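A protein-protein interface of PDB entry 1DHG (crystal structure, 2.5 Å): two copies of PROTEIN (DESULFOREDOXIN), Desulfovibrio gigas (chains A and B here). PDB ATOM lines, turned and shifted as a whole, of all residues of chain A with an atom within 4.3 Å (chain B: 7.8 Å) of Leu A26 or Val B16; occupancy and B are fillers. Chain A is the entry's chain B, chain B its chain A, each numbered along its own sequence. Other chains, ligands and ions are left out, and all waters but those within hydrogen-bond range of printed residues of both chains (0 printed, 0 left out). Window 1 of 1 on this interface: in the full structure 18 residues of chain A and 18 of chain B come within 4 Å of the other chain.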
ATOM      1  N   TYR A   7      18.655  12.459 -11.965  1.00  0.00           N
ATOM      2  CA  TYR A   7      18.720  12.421 -10.514  1.00  0.00           C
ATOM      3  C   TYR A   7      19.380  11.159  -9.987  1.00  0.00           C
ATOM      4  O   TYR A   7      19.177  10.064 -10.518  1.00  0.00           O
ATOM      5  CB  TYR A   7      17.316  12.567  -9.940  1.00  0.00           C
ATOM      6  CG  TYR A   7      16.816  13.987  -9.974  1.00  0.00           C
ATOM      7  CD1 TYR A   7      16.251  14.528 -11.135  1.00  0.00           C
ATOM      8  CD2 TYR A   7      16.923  14.802  -8.847  1.00  0.00           C
ATOM      9  CE1 TYR A   7      15.802  15.854 -11.166  1.00  0.00           C
ATOM     10  CE2 TYR A   7      16.482  16.123  -8.863  1.00  0.00           C
ATOM     11  CZ  TYR A   7      15.926  16.646 -10.022  1.00  0.00           C
ATOM     12  OH  TYR A   7      15.505  17.964 -10.024  1.00  0.00           O
ATOM     13  N   VAL A  16      18.202   8.043 -12.319  1.00  0.00           N
ATOM     14  CA  VAL A  16      17.029   8.058 -13.177  1.00  0.00           C
ATOM     15  C   VAL A  16      16.981   9.330 -14.004  1.00  0.00           C
ATOM     16  O   VAL A  16      17.558  10.346 -13.626  1.00  0.00           O
ATOM     17  CB  VAL A  16      15.701   7.927 -12.371  1.00  0.00           C
ATOM     18  CG1 VAL A  16      15.604   6.550 -11.707  1.00  0.00           C
ATOM     19  CG2 VAL A  16      15.598   9.035 -11.330  1.00  0.00           C
ATOM     20  N   LYS A  17      16.300   9.258 -15.140  1.00  0.00           N
ATOM     21  CA  LYS A  17      16.151  10.390 -16.041  1.00  0.00           C
ATOM     22  C   LYS A  17      14.665  10.745 -16.147  1.00  0.00           C
ATOM     23  O   LYS A  17      13.809   9.875 -16.329  1.00  0.00           O
ATOM     24  CB  LYS A  17      16.696  10.050 -17.435  1.00  0.00           C
ATOM     25  CG  LYS A  17      16.874  11.284 -18.322  1.00  0.00           C
ATOM     26  CD  LYS A  17      16.668  10.973 -19.791  1.00  0.00           C
ATOM     27  CE  LYS A  17      16.579  12.255 -20.597  1.00  0.00           C
ATOM     28  NZ  LYS A  17      16.051  11.980 -21.963  1.00  0.00           N
ATOM     29  N   VAL A  18      14.368  12.031 -16.044  1.00  0.00           N
ATOM     30  CA  VAL A  18      13.003  12.503 -16.113  1.00  0.00           C
ATOM     31  C   VAL A  18      12.483  12.502 -17.546  1.00  0.00           C
ATOM     32  O   VAL A  18      12.995  13.240 -18.383  1.00  0.00           O
ATOM     33  CB  VAL A  18      12.918  13.917 -15.525  1.00  0.00           C
ATOM     34  CG1 VAL A  18      11.506  14.445 -15.602  1.00  0.00           C
ATOM     35  CG2 VAL A  18      13.381  13.899 -14.094  1.00  0.00           C
ATOM     36  N   LEU A  19      11.496  11.650 -17.831  1.00  0.00           N
ATOM     37  CA  LEU A  19      10.883  11.569 -19.165  1.00  0.00           C
ATOM     38  C   LEU A  19       9.728  12.569 -19.290  1.00  0.00           C
ATOM     39  O   LEU A  19       9.588  13.235 -20.320  1.00  0.00           O
ATOM     40  CB  LEU A  19      10.382  10.148 -19.470  1.00  0.00           C
ATOM     41  CG  LEU A  19      11.391   9.002 -19.632  1.00  0.00           C
ATOM     42  CD1 LEU A  19      10.637   7.711 -19.843  1.00  0.00           C
ATOM     43  CD2 LEU A  19      12.343   9.248 -20.797  1.00  0.00           C
ATOM     44  N   GLY A  24       6.094  16.920  -8.254  1.00  0.00           N
ATOM     45  CA  GLY A  24       6.567  16.258  -7.051  1.00  0.00           C
ATOM     46  C   GLY A  24       8.076  16.130  -6.969  1.00  0.00           C
ATOM     47  O   GLY A  24       8.773  16.145  -7.986  1.00  0.00           O
ATOM     48  N   THR A  25       8.576  15.997  -5.748  1.00  0.00           N
ATOM     49  CA  THR A  25      10.003  15.853  -5.502  1.00  0.00           C
ATOM     50  C   THR A  25      10.374  14.367  -5.499  1.00  0.00           C
ATOM     51  O   THR A  25       9.718  13.559  -4.822  1.00  0.00           O
ATOM     52  CB  THR A  25      10.374  16.507  -4.168  1.00  0.00           C
ATOM     53  OG1 THR A  25      10.047  17.900  -4.231  1.00  0.00           O
ATOM     54  CG2 THR A  25      11.847  16.345  -3.869  1.00  0.00           C
ATOM     55  N   LEU A  26      11.396  14.014  -6.286  1.00  0.00           N
ATOM     56  CA  LEU A  26      11.857  12.633  -6.416  1.00  0.00           C
ATOM     57  C   LEU A  26      12.608  12.169  -5.178  1.00  0.00           C
ATOM     58  O   LEU A  26      13.598  12.783  -4.769  1.00  0.00           O
ATOM     59  CB  LEU A  26      12.714  12.483  -7.673  1.00  0.00           C
ATOM     60  CG  LEU A  26      12.016  12.680  -9.019  1.00  0.00           C
ATOM     61  CD1 LEU A  26      13.013  12.989 -10.100  1.00  0.00           C
ATOM     62  CD2 LEU A  26      11.256  11.439  -9.383  1.00  0.00           C
ATOM     63  N   VAL A  27      12.126  11.068  -4.610  1.00  0.00           N
ATOM     64  CA  VAL A  27      12.662  10.462  -3.386  1.00  0.00           C
ATOM     65  C   VAL A  27      13.091   9.003  -3.624  1.00  0.00           C
ATOM     66  O   VAL A  27      12.481   8.297  -4.410  1.00  0.00           O
ATOM     67  CB  VAL A  27      11.558  10.491  -2.260  1.00  0.00           C
ATOM     68  CG1 VAL A  27      11.969   9.666  -1.047  1.00  0.00           C
ATOM     69  CG2 VAL A  27      11.255  11.919  -1.853  1.00  0.00           C
ATOM     70  N   ASP A  32      15.743  12.640  -0.543  1.00  0.00           N
ATOM     71  CA  ASP A  32      15.568  13.389  -1.777  1.00  0.00           C
ATOM     72  C   ASP A  32      16.702  13.029  -2.735  1.00  0.00           C
ATOM     73  O   ASP A  32      17.872  13.011  -2.336  1.00  0.00           O
ATOM     74  CB  ASP A  32      15.651  14.894  -1.489  1.00  0.00           C
ATOM     75  CG  ASP A  32      14.297  15.529  -1.214  1.00  0.00           C
ATOM     76  OD1 ASP A  32      13.315  14.806  -0.922  1.00  0.00           O
ATOM     77  OD2 ASP A  32      14.215  16.776  -1.295  1.00  0.00           O
ATOM     78  N   MET A  33      16.361  12.725  -3.980  1.00  0.00           N
ATOM     79  CA  MET A  33      17.372  12.413  -4.969  1.00  0.00           C
ATOM     80  C   MET A  33      18.050  13.731  -5.326  1.00  0.00           C
ATOM     81  O   MET A  33      17.429  14.789  -5.238  1.00  0.00           O
ATOM     82  CB  MET A  33      16.729  11.766  -6.189  1.00  0.00           C
ATOM     83  CG  MET A  33      16.309  10.342  -5.925  1.00  0.00           C
ATOM     84  SD  MET A  33      15.509   9.555  -7.314  1.00  0.00           S
ATOM     85  CE  MET A  33      16.862   8.763  -8.111  1.00  0.00           C
ATOM     86  N   GLY B   4      16.511   0.616 -17.341  1.00  0.00           N
ATOM     87  CA  GLY B   4      15.609   0.700 -18.472  1.00  0.00           C
ATOM     88  C   GLY B   4      14.138   0.799 -18.085  1.00  0.00           C
ATOM     89  O   GLY B   4      13.329   1.306 -18.865  1.00  0.00           O
ATOM     90  N   ASP B   5      13.785   0.329 -16.889  1.00  0.00           N
ATOM     91  CA  ASP B   5      12.402   0.377 -16.427  1.00  0.00           C
ATOM     92  C   ASP B   5      11.892   1.808 -16.333  1.00  0.00           C
ATOM     93  O   ASP B   5      12.655   2.737 -16.069  1.00  0.00           O
ATOM     94  CB  ASP B   5      12.265  -0.302 -15.064  1.00  0.00           C
ATOM     95  CG  ASP B   5      12.467  -1.810 -15.128  1.00  0.00           C
ATOM     96  OD1 ASP B   5      12.288  -2.422 -16.214  1.00  0.00           O
ATOM     97  OD2 ASP B   5      12.786  -2.384 -14.064  1.00  0.00           O
ATOM     98  N   VAL B   6      10.591   1.974 -16.546  1.00  0.00           N
ATOM     99  CA  VAL B   6       9.962   3.288 -16.489  1.00  0.00           C
ATOM    100  C   VAL B   6       8.984   3.365 -15.333  1.00  0.00           C
ATOM    101  O   VAL B   6       8.178   2.459 -15.146  1.00  0.00           O
ATOM    102  CB  VAL B   6       9.181   3.573 -17.768  1.00  0.00           C
ATOM    103  CG1 VAL B   6       8.550   4.951 -17.695  1.00  0.00           C
ATOM    104  CG2 VAL B   6      10.104   3.470 -18.970  1.00  0.00           C
ATOM    105  N   TYR B   7       9.068   4.425 -14.539  1.00  0.00           N
ATOM    106  CA  TYR B   7       8.158   4.585 -13.410  1.00  0.00           C
ATOM    107  C   TYR B   7       7.368   5.867 -13.512  1.00  0.00           C
ATOM    108  O   TYR B   7       7.884   6.905 -13.956  1.00  0.00           O
ATOM    109  CB  TYR B   7       8.900   4.543 -12.079  1.00  0.00           C
ATOM    110  CG  TYR B   7       9.362   3.162 -11.712  1.00  0.00           C
ATOM    111  CD1 TYR B   7      10.423   2.568 -12.391  1.00  0.00           C
ATOM    112  CD2 TYR B   7       8.724   2.425 -10.709  1.00  0.00           C
ATOM    113  CE1 TYR B   7      10.838   1.271 -12.091  1.00  0.00           C
ATOM    114  CE2 TYR B   7       9.137   1.123 -10.395  1.00  0.00           C
ATOM    115  CZ  TYR B   7      10.196   0.555 -11.098  1.00  0.00           C
ATOM    116  OH  TYR B   7      10.609  -0.737 -10.860  1.00  0.00           O
ATOM    117  N   LYS B   8       6.098   5.781 -13.129  1.00  0.00           N
ATOM    118  CA  LYS B   8       5.217   6.934 -13.172  1.00  0.00           C
ATOM    119  C   LYS B   8       4.620   7.196 -11.805  1.00  0.00           C
ATOM    120  O   LYS B   8       4.357   6.269 -11.042  1.00  0.00           O
ATOM    121  CB  LYS B   8       4.089   6.725 -14.185  1.00  0.00           C
ATOM    122  CG  LYS B   8       3.184   7.941 -14.284  1.00  0.00           C
ATOM    123  CD  LYS B   8       2.204   7.911 -15.437  1.00  0.00           C
ATOM    124  CE  LYS B   8       1.656   9.324 -15.648  1.00  0.00           C
ATOM    125  NZ  LYS B   8       0.859   9.525 -16.893  1.00  0.00           N
ATOM    126  N   CYS B   9       4.454   8.471 -11.484  1.00  0.00           N
ATOM    127  CA  CYS B   9       3.862   8.883 -10.228  1.00  0.00           C
ATOM    128  C   CYS B   9       2.430   9.266 -10.553  1.00  0.00           C
ATOM    129  O   CYS B   9       2.204  10.295 -11.198  1.00  0.00           O
ATOM    130  CB  CYS B   9       4.582  10.109  -9.705  1.00  0.00           C
ATOM    131  SG  CYS B   9       3.552  11.027  -8.539  1.00  0.00           S
ATOM    132  N   CYS B  12       1.079  13.166  -9.747  1.00  0.00           N
ATOM    133  CA  CYS B  12       1.458  14.344 -10.529  1.00  0.00           C
ATOM    134  C   CYS B  12       1.879  14.002 -11.950  1.00  0.00           C
ATOM    135  O   CYS B  12       2.256  14.881 -12.713  1.00  0.00           O
ATOM    136  CB  CYS B  12       2.545  15.171  -9.838  1.00  0.00           C
ATOM    137  SG  CYS B  12       4.255  14.663 -10.189  1.00  0.00           S
ATOM    138  N   GLY B  13       1.841  12.716 -12.281  1.00  0.00           N
ATOM    139  CA  GLY B  13       2.190  12.278 -13.617  1.00  0.00           C
ATOM    140  C   GLY B  13       3.639  12.366 -14.065  1.00  0.00           C
ATOM    141  O   GLY B  13       3.917  12.271 -15.262  1.00  0.00           O
ATOM    142  N   GLN B  14       4.563  12.550 -13.127  1.00  0.00           N
ATOM    143  CA  GLN B  14       5.979  12.617 -13.467  1.00  0.00           C
ATOM    144  C   GLN B  14       6.431  11.210 -13.868  1.00  0.00           C
ATOM    145  O   GLN B  14       6.115  10.238 -13.177  1.00  0.00           O
ATOM    146  CB  GLN B  14       6.794  13.133 -12.265  1.00  0.00           C
ATOM    147  CG  GLN B  14       8.314  13.184 -12.496  1.00  0.00           C
ATOM    148  CD  GLN B  14       9.031  14.192 -11.607  1.00  0.00           C
ATOM    149  OE1 GLN B  14       9.526  15.202 -12.089  1.00  0.00           O
ATOM    150  NE2 GLN B  14       9.106  13.913 -10.316  1.00  0.00           N
ATOM    151  N   VAL B  15       7.132  11.104 -14.994  1.00  0.00           N
ATOM    152  CA  VAL B  15       7.620   9.815 -15.478  1.00  0.00           C
ATOM    153  C   VAL B  15       9.144   9.859 -15.522  1.00  0.00           C
ATOM    154  O   VAL B  15       9.724  10.867 -15.943  1.00  0.00           O
ATOM    155  CB  VAL B  15       7.083   9.501 -16.894  1.00  0.00           C
ATOM    156  CG1 VAL B  15       7.571   8.142 -17.342  1.00  0.00           C
ATOM    157  CG2 VAL B  15       5.563   9.553 -16.915  1.00  0.00           C
ATOM    158  N   VAL B  16       9.793   8.791 -15.061  1.00  0.00           N
ATOM    159  CA  VAL B  16      11.256   8.727 -15.059  1.00  0.00           C
ATOM    160  C   VAL B  16      11.724   7.377 -15.588  1.00  0.00           C
ATOM    161  O   VAL B  16      10.994   6.387 -15.498  1.00  0.00           O
ATOM    162  CB  VAL B  16      11.879   8.971 -13.624  1.00  0.00           C
ATOM    163  CG1 VAL B  16      11.421  10.298 -13.054  1.00  0.00           C
ATOM    164  CG2 VAL B  16      11.570   7.830 -12.676  1.00  0.00           C
ATOM    165  N   LYS B  17      12.935   7.344 -16.133  1.00  0.00           N
ATOM    166  CA  LYS B  17      13.523   6.122 -16.679  1.00  0.00           C
ATOM    167  C   LYS B  17      14.794   5.804 -15.884  1.00  0.00           C
ATOM    168  O   LYS B  17      15.619   6.691 -15.638  1.00  0.00           O
ATOM    169  CB  LYS B  17      13.861   6.343 -18.154  1.00  0.00           C
ATOM    170  CG  LYS B  17      14.393   5.145 -18.908  1.00  0.00           C
ATOM    171  CD  LYS B  17      14.868   5.630 -20.259  1.00  0.00           C
ATOM    172  CE  LYS B  17      15.245   4.496 -21.182  1.00  0.00           C
ATOM    173  NZ  LYS B  17      15.737   5.038 -22.488  1.00  0.00           N
ATOM    174  N   VAL B  18      14.944   4.553 -15.460  1.00  0.00           N
ATOM    175  CA  VAL B  18      16.119   4.163 -14.683  1.00  0.00           C
ATOM    176  C   VAL B  18      17.353   3.993 -15.561  1.00  0.00           C
ATOM    177  O   VAL B  18      17.387   3.145 -16.462  1.00  0.00           O
ATOM    178  CB  VAL B  18      15.878   2.864 -13.881  1.00  0.00           C
ATOM    179  CG1 VAL B  18      17.109   2.509 -13.071  1.00  0.00           C
ATOM    180  CG2 VAL B  18      14.684   3.029 -12.967  1.00  0.00           C
ATOM    181  N   LEU B  19      18.347   4.838 -15.313  1.00  0.00           N
ATOM    182  CA  LEU B  19      19.611   4.795 -16.061  1.00  0.00           C
ATOM    183  C   LEU B  19      20.604   3.833 -15.382  1.00  0.00           C
ATOM    184  O   LEU B  19      21.281   3.045 -16.053  1.00  0.00           O
ATOM    185  CB  LEU B  19      20.215   6.204 -16.185  1.00  0.00           C
ATOM    186  CG  LEU B  19      19.275   7.234 -16.816  1.00  0.00           C
ATOM    187  CD1 LEU B  19      19.893   8.604 -16.780  1.00  0.00           C
ATOM    188  CD2 LEU B  19      18.914   6.836 -18.237  1.00  0.00           C
ATOM    189  N   LEU B  26      11.651   3.762  -5.656  1.00  0.00           N
ATOM    190  CA  LEU B  26      11.391   5.101  -6.174  1.00  0.00           C
ATOM    191  C   LEU B  26      10.101   5.678  -5.627  1.00  0.00           C
ATOM    192  O   LEU B  26       9.033   5.079  -5.789  1.00  0.00           O
ATOM    193  CB  LEU B  26      11.322   5.093  -7.709  1.00  0.00           C
ATOM    194  CG  LEU B  26      12.596   4.802  -8.510  1.00  0.00           C
ATOM    195  CD1 LEU B  26      12.297   4.854  -9.995  1.00  0.00           C
ATOM    196  CD2 LEU B  26      13.675   5.802  -8.146  1.00  0.00           C
ATOM    197  N   VAL B  27      10.211   6.847  -5.004  1.00  0.00           N
ATOM    198  CA  VAL B  27       9.084   7.569  -4.407  1.00  0.00           C
ATOM    199  C   VAL B  27       8.953   8.968  -5.025  1.00  0.00           C
ATOM    200  O   VAL B  27       9.952   9.577  -5.419  1.00  0.00           O
ATOM    201  CB  VAL B  27       9.274   7.736  -2.873  1.00  0.00           C
ATOM    202  CG1 VAL B  27       8.236   8.674  -2.297  1.00  0.00           C
ATOM    203  CG2 VAL B  27       9.209   6.389  -2.178  1.00  0.00           C
ATOM    204  N   CYS B  28       7.721   9.464  -5.122  1.00  0.00           N
ATOM    205  CA  CYS B  28       7.445  10.796  -5.656  1.00  0.00           C
ATOM    206  C   CYS B  28       6.104  11.226  -5.066  1.00  0.00           C
ATOM    207  O   CYS B  28       5.183  10.411  -4.978  1.00  0.00           O
ATOM    208  CB  CYS B  28       7.376  10.765  -7.180  1.00  0.00           C
ATOM    209  SG  CYS B  28       7.263  12.426  -7.918  1.00  0.00           S
ATOM    210  N   CYS B  29       5.991  12.492  -4.661  1.00  0.00           N
ATOM    211  CA  CYS B  29       4.759  13.000  -4.035  1.00  0.00           C
ATOM    212  C   CYS B  29       4.393  12.112  -2.839  1.00  0.00           C
ATOM    213  O   CYS B  29       3.216  11.837  -2.581  1.00  0.00           O
ATOM    214  CB  CYS B  29       3.585  13.067  -5.022  1.00  0.00           C
ATOM    215  SG  CYS B  29       3.640  14.457  -6.189  1.00  0.00           S
ATOM    216  N   GLY B  30       5.424  11.634  -2.143  1.00  0.00           N
ATOM    217  CA  GLY B  30       5.238  10.791  -0.983  1.00  0.00           C
ATOM    218  C   GLY B  30       4.733   9.390  -1.253  1.00  0.00           C
ATOM    219  O   GLY B  30       4.581   8.609  -0.313  1.00  0.00           O
ATOM    220  N   MET B  33       6.351   5.127  -6.786  1.00  0.00           N
ATOM    221  CA  MET B  33       6.080   5.275  -8.209  1.00  0.00           C
ATOM    222  C   MET B  33       5.696   3.900  -8.737  1.00  0.00           C
ATOM    223  O   MET B  33       6.147   2.881  -8.212  1.00  0.00           O
ATOM    224  CB  MET B  33       7.299   5.820  -8.955  1.00  0.00           C
ATOM    225  CG  MET B  33       7.571   7.282  -8.644  1.00  0.00           C
ATOM    226  SD  MET B  33       8.872   8.013  -9.637  1.00  0.00           S
ATOM    227  CE  MET B  33       7.944   8.992 -10.810  1.00  0.00           C
ATOM    228  N   VAL B  34       4.837   3.873  -9.748  1.00  0.00           N
ATOM    229  CA  VAL B  34       4.370   2.623 -10.344  1.00  0.00           C
ATOM    230  C   VAL B  34       5.207   2.210 -11.549  1.00  0.00           C
ATOM    231  O   VAL B  34       5.506   3.031 -12.419  1.00  0.00           O
ATOM    232  CB  VAL B  34       2.916   2.755 -10.823  1.00  0.00           C
ATOM    233  CG1 VAL B  34       2.382   1.386 -11.226  1.00  0.00           C
ATOM    234  CG2 VAL B  34       2.055   3.396  -9.749  1.00  0.00           C
ATOM    235  N   GLN B  36       5.864   0.915 -15.038  1.00  0.00           N
ATOM    236  CA  GLN B  36       5.050   0.894 -16.241  1.00  0.00           C
ATOM    237  C   GLN B  36       5.351  -0.338 -17.085  1.00  0.00           C
ATOM    238  O   GLN B  36       4.431  -0.795 -17.795  1.00  0.00           O
ATOM    239  CB  GLN B  36       5.257   2.173 -17.053  1.00  0.00           C
ATOM    240  CG  GLN B  36       4.886   3.448 -16.303  1.00  0.00           C
ATOM    241  CD  GLN B  36       3.465   3.417 -15.770  1.00  0.00           C
ATOM    242  OE1 GLN B  36       3.227   3.080 -14.607  1.00  0.00           O
ATOM    243  NE2 GLN B  36       2.509   3.779 -16.618  1.00  0.00           N
ATOM    244  OXT GLN B  36       6.489  -0.857 -16.991  1.00  0.00           O
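Of the printed residues of chain B, Lys A17 touches Val B16, Lys B17 and Leu B19. Of the printed residues of chain B, Val A18 touches Val B15 (3.6 Å). Printed residues of chain B within 4 Å of Leu A26: Gln B14 (3.4 Å), Val B16 (3.8 Å) and Val B27 (3.7 Å). Met A33 touches none of the printed residues of chain B. Tyr B7 touches none of the printed residues of chain A. Printed residues of chain A within 4 Å of Gln B14: Gly A24 and Leu A26. Val B16 touches two residues of chain A. Of the printed residues of chain A, Lys B17 touches Val A16, Lys A17 and Leu A19. Of the printed residues of chain A, Cys B28 touches Gly A24 (3.9 Å) and Thr A25 (3.7 Å). The nearest residue of chain B that does not touch Leu A26 is Met B33 (4.2 Å). The nearest residue of chain A that does not touch Val B16 is Leu A19 (4.04 Å).
The backbone NH (N) of Gly B4 lies within hydrogen-bond range of the backbone carbonyl oxygen (O) of Val B18, 2.8 Å away. N of Val B16 lies within hydrogen-bond range of O of Tyr B7, 2.9 Å away. The backbone NH (N) of Cys B9 lies within hydrogen-bond range of the backbone carbonyl oxygen (O) of Gln B14, 3.0 Å away. The side-chain sulfur (SG) of Cys B12 lies close to the backbone NH (N) of Gln B14, 3.6 Å away. The backbone NH of Met B33 lies within hydrogen-bond range of the backbone carbonyl oxygen of Leu B26, 2.9 Å away. N of Met A33 sits at hydrogen-bond distance from O of Leu A26.
Val A16 touches Val B18. Lys A17 touches Val B16 (O to CA, 3.1 Å). Lys A17 touches Leu B19 (CB to CD1, 3.6 Å). Val B15 touches Val A18 (O to C, 3.6 Å). Leu A19 touches Lys B17 (CD1 to CB, 3.9 Å). Gly A24 touches Cys B28. Cys B28 touches Thr A25. Thr A25 touches Cys B29 (O to N, 3.9 Å). Gln B14 touches Leu A26 (NE2 to CD2, 3.4 Å). Leu A26 touches Val B27 (C to O, 3.7 Å).
Printed residues of chain A that touch a printed residue of chain B: Val A16, Lys A17, Val A18, Leu A19, Gly A24, Thr A25, Leu A26 and Val A27. Hydrophobic or aromatic side chains of chain A within 4 Å of the printed part of chain B: Val A16, Leu A19, Leu A26 and Val A27. Along chain A the printed residues that touch a printed residue of chain B span positions 16 to 27. Of the 22 printed residues of chain B, 11 touch a printed residue of chain A. Printed residues of chain B that touch a printed residue of chain A: Cys B12, Gln B14, Val B15, Val B16, Lys B17, Val B18, Leu B19, Leu B26, Val B27, Cys B28 and Cys B29. Hydrophobic or aromatic side chains of chain B that line the printed part of chain A: Val B15, Val B16, Val B18, Leu B19 and Val B27.
Val A16 touches Val B18, but with the chains exchanged Val A18 does not touch Val B16 (4.1 Å). Lys A17 touches Leu B19, and with the chains exchanged Leu A19 touches Lys B17. Leu A26 touches Val B27, and with the chains exchanged Val A27 touches Leu B26. Val B27 touches its own counterpart, Val A27. Positions printed for both chains: 7, 16, 17, 18, 19, 26, 27 and 33.
The side-chain sulfur (SG) of Cys B12 sits close to the backbone NH (N) of Gly A24 (3.5 Å). The backbone carbonyl oxygen of Gly A24 lies within hydrogen-bond range of the side-chain amide nitrogen of Gln B14, at 3.2 Å. The backbone NH of Leu A19 lies within hydrogen-bond range of the backbone carbonyl oxygen of Val B15 (2.7 Å). N of Lys B17 lies within hydrogen-bond range of O of Lys A17, 2.7 Å away. N of Val B27 sits at hydrogen-bond distance from O of Val A27, 2.8 Å away.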
